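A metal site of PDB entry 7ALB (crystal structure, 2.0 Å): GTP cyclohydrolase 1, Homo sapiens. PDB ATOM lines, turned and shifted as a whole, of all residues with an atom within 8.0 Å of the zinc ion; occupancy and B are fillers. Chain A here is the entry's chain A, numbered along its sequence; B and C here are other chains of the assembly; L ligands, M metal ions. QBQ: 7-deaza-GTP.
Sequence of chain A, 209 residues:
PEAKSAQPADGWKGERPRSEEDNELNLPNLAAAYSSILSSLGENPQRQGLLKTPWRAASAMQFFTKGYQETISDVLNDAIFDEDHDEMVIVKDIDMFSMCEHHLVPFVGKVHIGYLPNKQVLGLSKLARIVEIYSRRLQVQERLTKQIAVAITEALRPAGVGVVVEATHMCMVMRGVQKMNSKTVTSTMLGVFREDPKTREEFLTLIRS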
ATOM      1  N   MET A  99     -17.246 -22.013   7.885  1.00  0.00           N
ATOM      2  CA  MET A  99     -15.810 -22.115   8.061  1.00  0.00           C
ATOM      3  C   MET A  99     -15.446 -23.488   8.615  1.00  0.00           C
ATOM      4  O   MET A  99     -15.919 -23.878   9.690  1.00  0.00           O
ATOM      5  CB  MET A  99     -15.316 -21.029   9.037  1.00  0.00           C
ATOM      6  CG  MET A  99     -15.276 -19.644   8.428  1.00  0.00           C
ATOM      7  SD  MET A  99     -13.998 -19.514   7.137  1.00  0.00           S
ATOM      8  CE  MET A  99     -12.644 -19.682   8.082  1.00  0.00           C
ATOM      9  N   CYS A 100     -14.592 -24.204   7.906  1.00  0.00           N
ATOM     10  CA  CYS A 100     -14.136 -25.503   8.363  1.00  0.00           C
ATOM     11  C   CYS A 100     -13.323 -25.306   9.643  1.00  0.00           C
ATOM     12  O   CYS A 100     -12.411 -24.492   9.667  1.00  0.00           O
ATOM     13  CB  CYS A 100     -13.288 -26.159   7.299  1.00  0.00           C
ATOM     14  SG  CYS A 100     -12.169 -27.368   8.008  1.00  0.00           S
ATOM     15  N   GLU A 101     -13.629 -26.046  10.692  1.00  0.00           N
ATOM     16  CA  GLU A 101     -12.899 -25.839  11.970  1.00  0.00           C
ATOM     17  C   GLU A 101     -11.503 -26.483  12.001  1.00  0.00           C
ATOM     18  O   GLU A 101     -10.705 -26.144  12.851  1.00  0.00           O
ATOM     19  CB  GLU A 101     -13.730 -26.330  13.154  1.00  0.00           C
ATOM     20  CG  GLU A 101     -13.853 -27.834  13.242  1.00  0.00           C
ATOM     21  CD  GLU A 101     -14.819 -28.301  14.315  1.00  0.00           C
ATOM     22  OE1 GLU A 101     -14.764 -29.495  14.678  1.00  0.00           O
ATOM     23  OE2 GLU A 101     -15.633 -27.480  14.785  1.00  0.00           O
ATOM     24  N   HIS A 102     -11.247 -27.391  11.065  1.00  0.00           N
ATOM     25  CA  HIS A 102      -9.983 -28.078  10.983  1.00  0.00           C
ATOM     26  C   HIS A 102      -8.906 -27.246  10.281  1.00  0.00           C
ATOM     27  O   HIS A 102      -7.745 -27.299  10.655  1.00  0.00           O
ATOM     28  CB  HIS A 102     -10.152 -29.408  10.264  1.00  0.00           C
ATOM     29  CG  HIS A 102     -10.976 -30.394  11.022  1.00  0.00           C
ATOM     30  ND1 HIS A 102     -10.420 -31.367  11.820  1.00  0.00           N
ATOM     31  CD2 HIS A 102     -12.315 -30.548  11.122  1.00  0.00           C
ATOM     32  CE1 HIS A 102     -11.377 -32.079  12.378  1.00  0.00           C
ATOM     33  NE2 HIS A 102     -12.542 -31.604  11.963  1.00  0.00           N
ATOM     34  N   HIS A 103      -9.319 -26.492   9.270  1.00  0.00           N
ATOM     35  CA  HIS A 103      -8.376 -25.711   8.497  1.00  0.00           C
ATOM     36  C   HIS A 103      -8.598 -24.197   8.480  1.00  0.00           C
ATOM     37  O   HIS A 103      -7.749 -23.509   7.948  1.00  0.00           O
ATOM     38  CB  HIS A 103      -8.363 -26.199   7.048  1.00  0.00           C
ATOM     39  CG  HIS A 103      -7.798 -27.567   6.860  1.00  0.00           C
ATOM     40  ND1 HIS A 103      -8.596 -28.679   6.661  1.00  0.00           N
ATOM     41  CD2 HIS A 103      -6.523 -28.016   6.814  1.00  0.00           C
ATOM     42  CE1 HIS A 103      -7.836 -29.745   6.518  1.00  0.00           C
ATOM     43  NE2 HIS A 103      -6.573 -29.370   6.600  1.00  0.00           N
ATOM     44  N   LEU A 104      -9.722 -23.724   9.029  1.00  0.00           N
ATOM     45  CA  LEU A 104     -10.073 -22.296   9.027  1.00  0.00           C
ATOM     46  C   LEU A 104     -10.155 -21.751   7.600  1.00  0.00           C
ATOM     47  O   LEU A 104      -9.613 -20.685   7.292  1.00  0.00           O
ATOM     48  CB  LEU A 104      -9.156 -21.427   9.904  1.00  0.00           C
ATOM     49  CG  LEU A 104      -9.051 -21.844  11.365  1.00  0.00           C
ATOM     50  CD1 LEU A 104      -8.117 -20.914  12.133  1.00  0.00           C
ATOM     51  CD2 LEU A 104     -10.413 -21.908  12.026  1.00  0.00           C
ATOM     52  N   VAL A 105     -10.810 -22.531   6.725  1.00  0.00           N
ATOM     53  CA  VAL A 105     -10.983 -22.219   5.310  1.00  0.00           C
ATOM     54  C   VAL A 105     -12.499 -22.416   5.016  1.00  0.00           C
ATOM     55  O   VAL A 105     -13.130 -23.302   5.591  1.00  0.00           O
ATOM     56  CB  VAL A 105     -10.100 -23.182   4.482  1.00  0.00           C
ATOM     57  CG1 VAL A 105     -10.448 -23.163   2.992  1.00  0.00           C
ATOM     58  CG2 VAL A 105      -8.603 -22.890   4.713  1.00  0.00           C
ATOM     59  N   PRO A 106     -13.113 -21.561   4.175  1.00  0.00           N
ATOM     60  CA  PRO A 106     -14.567 -21.706   3.923  1.00  0.00           C
ATOM     61  C   PRO A 106     -15.054 -23.002   3.273  1.00  0.00           C
ATOM     62  O   PRO A 106     -14.373 -23.622   2.458  1.00  0.00           O
ATOM     63  CB  PRO A 106     -14.898 -20.532   2.981  1.00  0.00           C
ATOM     64  CG  PRO A 106     -13.745 -19.569   3.119  1.00  0.00           C
ATOM     65  CD  PRO A 106     -12.535 -20.427   3.436  1.00  0.00           C
ATOM     66  N   PHE A 107     -16.270 -23.362   3.590  1.00  0.00           N
ATOM     67  CA  PHE A 107     -17.037 -24.408   2.913  1.00  0.00           C
ATOM     68  C   PHE A 107     -18.377 -23.761   2.599  1.00  0.00           C
ATOM     69  O   PHE A 107     -18.963 -23.099   3.463  1.00  0.00           O
ATOM     70  CB  PHE A 107     -17.107 -25.778   3.621  1.00  0.00           C
ATOM     71  CG  PHE A 107     -17.898 -25.942   4.899  1.00  0.00           C
ATOM     72  CD1 PHE A 107     -19.192 -26.440   4.861  1.00  0.00           C
ATOM     73  CD2 PHE A 107     -17.291 -25.784   6.136  1.00  0.00           C
ATOM     74  CE1 PHE A 107     -19.889 -26.659   6.042  1.00  0.00           C
ATOM     75  CE2 PHE A 107     -17.989 -26.019   7.312  1.00  0.00           C
ATOM     76  CZ  PHE A 107     -19.281 -26.452   7.258  1.00  0.00           C
ATOM     77  N   GLN A 139     -17.109 -24.921  12.055  1.00  0.00           N
ATOM     78  CA  GLN A 139     -17.930 -26.109  11.975  1.00  0.00           C
ATOM     79  C   GLN A 139     -17.408 -27.304  11.212  1.00  0.00           C
ATOM     80  O   GLN A 139     -16.314 -27.314  10.683  1.00  0.00           O
ATOM     81  CB  GLN A 139     -19.203 -25.701  11.232  1.00  0.00           C
ATOM     82  CG  GLN A 139     -20.195 -24.902  12.030  1.00  0.00           C
ATOM     83  CD  GLN A 139     -21.068 -25.798  12.868  1.00  0.00           C
ATOM     84  OE1 GLN A 139     -20.814 -26.980  12.981  1.00  0.00           O
ATOM     85  NE2 GLN A 139     -22.103 -25.228  13.449  1.00  0.00           N
ATOM     86  N   HIS A 169     -16.184 -27.915  -0.219  1.00  0.00           N
ATOM     87  CA  HIS A 169     -15.244 -27.602   0.802  1.00  0.00           C
ATOM     88  C   HIS A 169     -14.022 -27.104   0.044  1.00  0.00           C
ATOM     89  O   HIS A 169     -13.444 -27.836  -0.739  1.00  0.00           O
ATOM     90  CB  HIS A 169     -14.943 -28.828   1.647  1.00  0.00           C
ATOM     91  CG  HIS A 169     -16.012 -29.153   2.652  1.00  0.00           C
ATOM     92  ND1 HIS A 169     -15.811 -29.059   4.001  1.00  0.00           N
ATOM     93  CD2 HIS A 169     -17.291 -29.548   2.489  1.00  0.00           C
ATOM     94  CE1 HIS A 169     -16.915 -29.397   4.637  1.00  0.00           C
ATOM     95  NE2 HIS A 169     -17.834 -29.686   3.742  1.00  0.00           N
ATOM     96  N   MET A 170     -13.582 -25.861   0.297  1.00  0.00           N
ATOM     97  CA  MET A 170     -12.394 -25.321  -0.346  1.00  0.00           C
ATOM     98  C   MET A 170     -11.109 -26.060   0.063  1.00  0.00           C
ATOM     99  O   MET A 170     -10.162 -26.100  -0.723  1.00  0.00           O
ATOM    100  CB  MET A 170     -12.281 -23.791  -0.153  1.00  0.00           C
ATOM    101  CG  MET A 170     -13.376 -23.012  -0.892  1.00  0.00           C
ATOM    102  SD  MET A 170     -13.351 -23.347  -2.680  1.00  0.00           S
ATOM    103  CE  MET A 170     -15.071 -23.012  -3.084  1.00  0.00           C
ATOM    104  N   CYS A 171     -11.080 -26.693   1.248  1.00  0.00           N
ATOM    105  CA  CYS A 171      -9.974 -27.519   1.677  1.00  0.00           C
ATOM    106  C   CYS A 171      -9.793 -28.801   0.823  1.00  0.00           C
ATOM    107  O   CYS A 171      -8.735 -29.402   0.884  1.00  0.00           O
ATOM    108  CB  CYS A 171     -10.122 -27.853   3.149  1.00  0.00           C
ATOM    109  SG  CYS A 171     -10.547 -26.430   4.146  1.00  0.00           S
ATOM    110  N   MET A 172     -10.818 -29.228   0.073  1.00  0.00           N
ATOM    111  CA  MET A 172     -10.697 -30.351  -0.832  1.00  0.00           C
ATOM    112  C   MET A 172     -10.494 -29.926  -2.286  1.00  0.00           C
ATOM    113  O   MET A 172     -10.273 -30.789  -3.120  1.00  0.00           O
ATOM    114  CB  MET A 172     -11.904 -31.288  -0.700  1.00  0.00           C
ATOM    115  CG  MET A 172     -11.960 -31.979   0.647  1.00  0.00           C
ATOM    116  SD  MET A 172     -13.408 -33.036   0.861  1.00  0.00           S
ATOM    117  CE  MET A 172     -13.203 -34.214  -0.493  1.00  0.00           C
ATOM    118  N   ARG A 175      -6.576 -27.213  -2.130  1.00  0.00           N
ATOM    119  CA  ARG A 175      -5.463 -27.882  -1.483  1.00  0.00           C
ATOM    120  C   ARG A 175      -5.792 -29.343  -1.162  1.00  0.00           C
ATOM    121  O   ARG A 175      -6.856 -29.829  -1.507  1.00  0.00           O
ATOM    122  CB  ARG A 175      -5.127 -27.164  -0.166  1.00  0.00           C
ATOM    123  CG  ARG A 175      -6.306 -27.073   0.791  1.00  0.00           C
ATOM    124  CD  ARG A 175      -5.905 -26.997   2.248  1.00  0.00           C
ATOM    125  NE  ARG A 175      -5.005 -28.074   2.642  1.00  0.00           N
ATOM    126  CZ  ARG A 175      -5.390 -29.283   2.997  1.00  0.00           C
ATOM    127  NH1 ARG A 175      -6.664 -29.607   3.001  1.00  0.00           N
ATOM    128  NH2 ARG A 175      -4.493 -30.189   3.338  1.00  0.00           N
ATOM    129  N   ARG B  56      -2.848 -27.255  11.180  1.00  0.00           N
ATOM    130  CA  ARG B  56      -3.473 -27.521   9.886  1.00  0.00           C
ATOM    131  C   ARG B  56      -3.801 -26.234   9.133  1.00  0.00           C
ATOM    132  O   ARG B  56      -3.687 -26.179   7.929  1.00  0.00           O
ATOM    133  CB  ARG B  56      -4.692 -28.424  10.061  1.00  0.00           C
ATOM    134  CG  ARG B  56      -4.322 -29.874  10.272  1.00  0.00           C
ATOM    135  CD  ARG B  56      -5.525 -30.720  10.599  1.00  0.00           C
ATOM    136  NE  ARG B  56      -6.367 -30.135  11.638  1.00  0.00           N
ATOM    137  CZ  ARG B  56      -7.196 -30.835  12.397  1.00  0.00           C
ATOM    138  NH1 ARG B  56      -7.287 -32.141  12.226  1.00  0.00           N
ATOM    139  NH2 ARG B  56      -7.932 -30.220  13.321  1.00  0.00           N
ATOM    140  N   ALA B  60      -2.041 -25.117   5.611  1.00  0.00           N
ATOM    141  CA  ALA B  60      -2.910 -24.725   4.503  1.00  0.00           C
ATOM    142  C   ALA B  60      -2.498 -23.340   3.989  1.00  0.00           C
ATOM    143  O   ALA B  60      -2.291 -23.185   2.786  1.00  0.00           O
ATOM    144  CB  ALA B  60      -4.375 -24.731   4.932  1.00  0.00           C
ATOM    145  N   LEU C 124     -13.783 -36.032   5.726  1.00  0.00           N
ATOM    146  CA  LEU C 124     -14.279 -35.867   4.355  1.00  0.00           C
ATOM    147  C   LEU C 124     -13.266 -36.148   3.253  1.00  0.00           C
ATOM    148  O   LEU C 124     -13.529 -36.930   2.350  1.00  0.00           O
ATOM    149  CB  LEU C 124     -14.909 -34.494   4.161  1.00  0.00           C
ATOM    150  CG  LEU C 124     -16.208 -34.243   4.931  1.00  0.00           C
ATOM    151  CD1 LEU C 124     -16.729 -32.850   4.687  1.00  0.00           C
ATOM    152  CD2 LEU C 124     -17.266 -35.284   4.604  1.00  0.00           C
ATOM    153  N   SER C 125     -12.097 -35.535   3.359  1.00  0.00           N
ATOM    154  CA  SER C 125     -11.040 -35.713   2.363  1.00  0.00           C
ATOM    155  C   SER C 125     -10.530 -37.156   2.237  1.00  0.00           C
ATOM    156  O   SER C 125     -10.127 -37.561   1.174  1.00  0.00           O
ATOM    157  CB  SER C 125      -9.883 -34.744   2.609  1.00  0.00           C
ATOM    158  OG  SER C 125      -9.028 -35.204   3.628  1.00  0.00           O
HETATM  159  O3  QBQ L   1      -5.107 -35.607   8.377  1.00  0.00           O
HETATM  160  C4  QBQ L   1     -12.675 -31.036   7.601  1.00  0.00           C
HETATM  161  C5  QBQ L   1     -11.634 -33.358   7.610  1.00  0.00           C
HETATM  162  O4  QBQ L   1      -5.633 -33.173   8.072  1.00  0.00           O
HETATM  163  C6  QBQ L   1      -9.704 -34.230   8.369  1.00  0.00           C
HETATM  164  N1  QBQ L   1     -14.404 -34.033   8.161  1.00  0.00           N
HETATM  165  C7  QBQ L   1      -8.445 -33.807   9.077  1.00  0.00           C
HETATM  166  C8  QBQ L   1      -9.638 -34.224   6.830  1.00  0.00           C
HETATM  167  N2  QBQ L   1     -12.724 -32.400   7.775  1.00  0.00           N
HETATM  168  C9  QBQ L   1     -10.689 -33.168   6.437  1.00  0.00           C
HETATM  169  O5  QBQ L   1      -4.926 -31.378   6.547  1.00  0.00           O
HETATM  170  C10 QBQ L   1     -16.239 -31.841   7.923  1.00  0.00           C
HETATM  171  O6  QBQ L   1      -3.756 -33.596   6.472  1.00  0.00           O
HETATM  172  N3  QBQ L   1     -16.597 -33.143   8.174  1.00  0.00           N
HETATM  173  O7  QBQ L   1      -6.074 -33.359   5.657  1.00  0.00           O
HETATM  174  O8  QBQ L   1      -4.994 -32.897   3.465  1.00  0.00           O
HETATM  175  N   QBQ L   1     -16.215 -35.389   8.530  1.00  0.00           N
HETATM  176  C   QBQ L   1     -15.715 -34.180   8.291  1.00  0.00           C
HETATM  177  O   QBQ L   1     -10.800 -33.365   8.735  1.00  0.00           O
HETATM  178  C1  QBQ L   1     -14.015 -32.770   7.931  1.00  0.00           C
HETATM  179  C2  QBQ L   1     -14.815 -31.651   7.818  1.00  0.00           C
HETATM  180  C3  QBQ L   1     -13.953 -30.540   7.618  1.00  0.00           C
HETATM  181  O1  QBQ L   1      -7.399 -34.739   8.732  1.00  0.00           O
HETATM  182  O10 QBQ L   1      -6.617 -34.619   3.641  1.00  0.00           O
HETATM  183  O11 QBQ L   1      -9.981 -35.517   6.338  1.00  0.00           O
HETATM  184  O12 QBQ L   1     -11.351 -33.453   5.223  1.00  0.00           O
HETATM  185  O13 QBQ L   1     -17.096 -30.986   7.763  1.00  0.00           O
HETATM  186  O2  QBQ L   1      -5.673 -34.187  10.290  1.00  0.00           O
HETATM  187  O9  QBQ L   1      -7.283 -32.346   3.868  1.00  0.00           O
HETATM  188  P   QBQ L   1      -5.882 -34.507   8.887  1.00  0.00           P
HETATM  189  P1  QBQ L   1      -4.972 -32.841   6.671  1.00  0.00           P
HETATM  190  P2  QBQ L   1      -6.198 -33.297   4.075  1.00  0.00           P
HETATM  191 ZN    ZN M   1     -10.927 -28.119   5.974  1.00  0.00          ZN
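A ring nitrogen (NE2) of His 103 is in hydrogen-bond range of an oxygen (O5) of the ligand (2.6 Å). The guanidinium group (NH2) of Arg 175 is in salt-bridge range of an oxygen (O8) of the ligand, 2.8 Å away. NH1 of Arg 56 of chain B lies within salt-bridge range of O2 of the ligand (3.2 Å). The backbone NH (N) of Ser 125 of chain C is in hydrogen-bond range of an oxygen (O12) of the ligand (2.9 Å). The side-chain hydroxyl (OG) of Ser 125 of chain C lies within hydrogen-bond range of an oxygen (O10) of the ligand (2.5 Å). The backbone NH (N) of Leu 124 of chain C is in hydrogen-bond range of a nitrogen (N1) of the ligand (3.2 Å).
N of His 102 sits close to SG of Cys 100, at 3.2 Å. O of Val 105 lies within hydrogen-bond range of N of Cys 100, at 2.9 Å. The guanidinium group of Arg 175 lies within hydrogen-bond range of the backbone carbonyl oxygen of Cys 171.
Within 4 Å of the zinc ion: Cys 100, His 103 and Cys 171.
A ring nitrogen (ND1) of His 103 binds the zinc ion (2.5 Å). The side-chain sulfur (SG) of Cys 100 is bound to the zinc ion, 2.5 Å away. The side-chain sulfur (SG) of Cys 171 binds the zinc ion, 2.5 Å away. The zinc ion has three donor atoms within binding distance.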
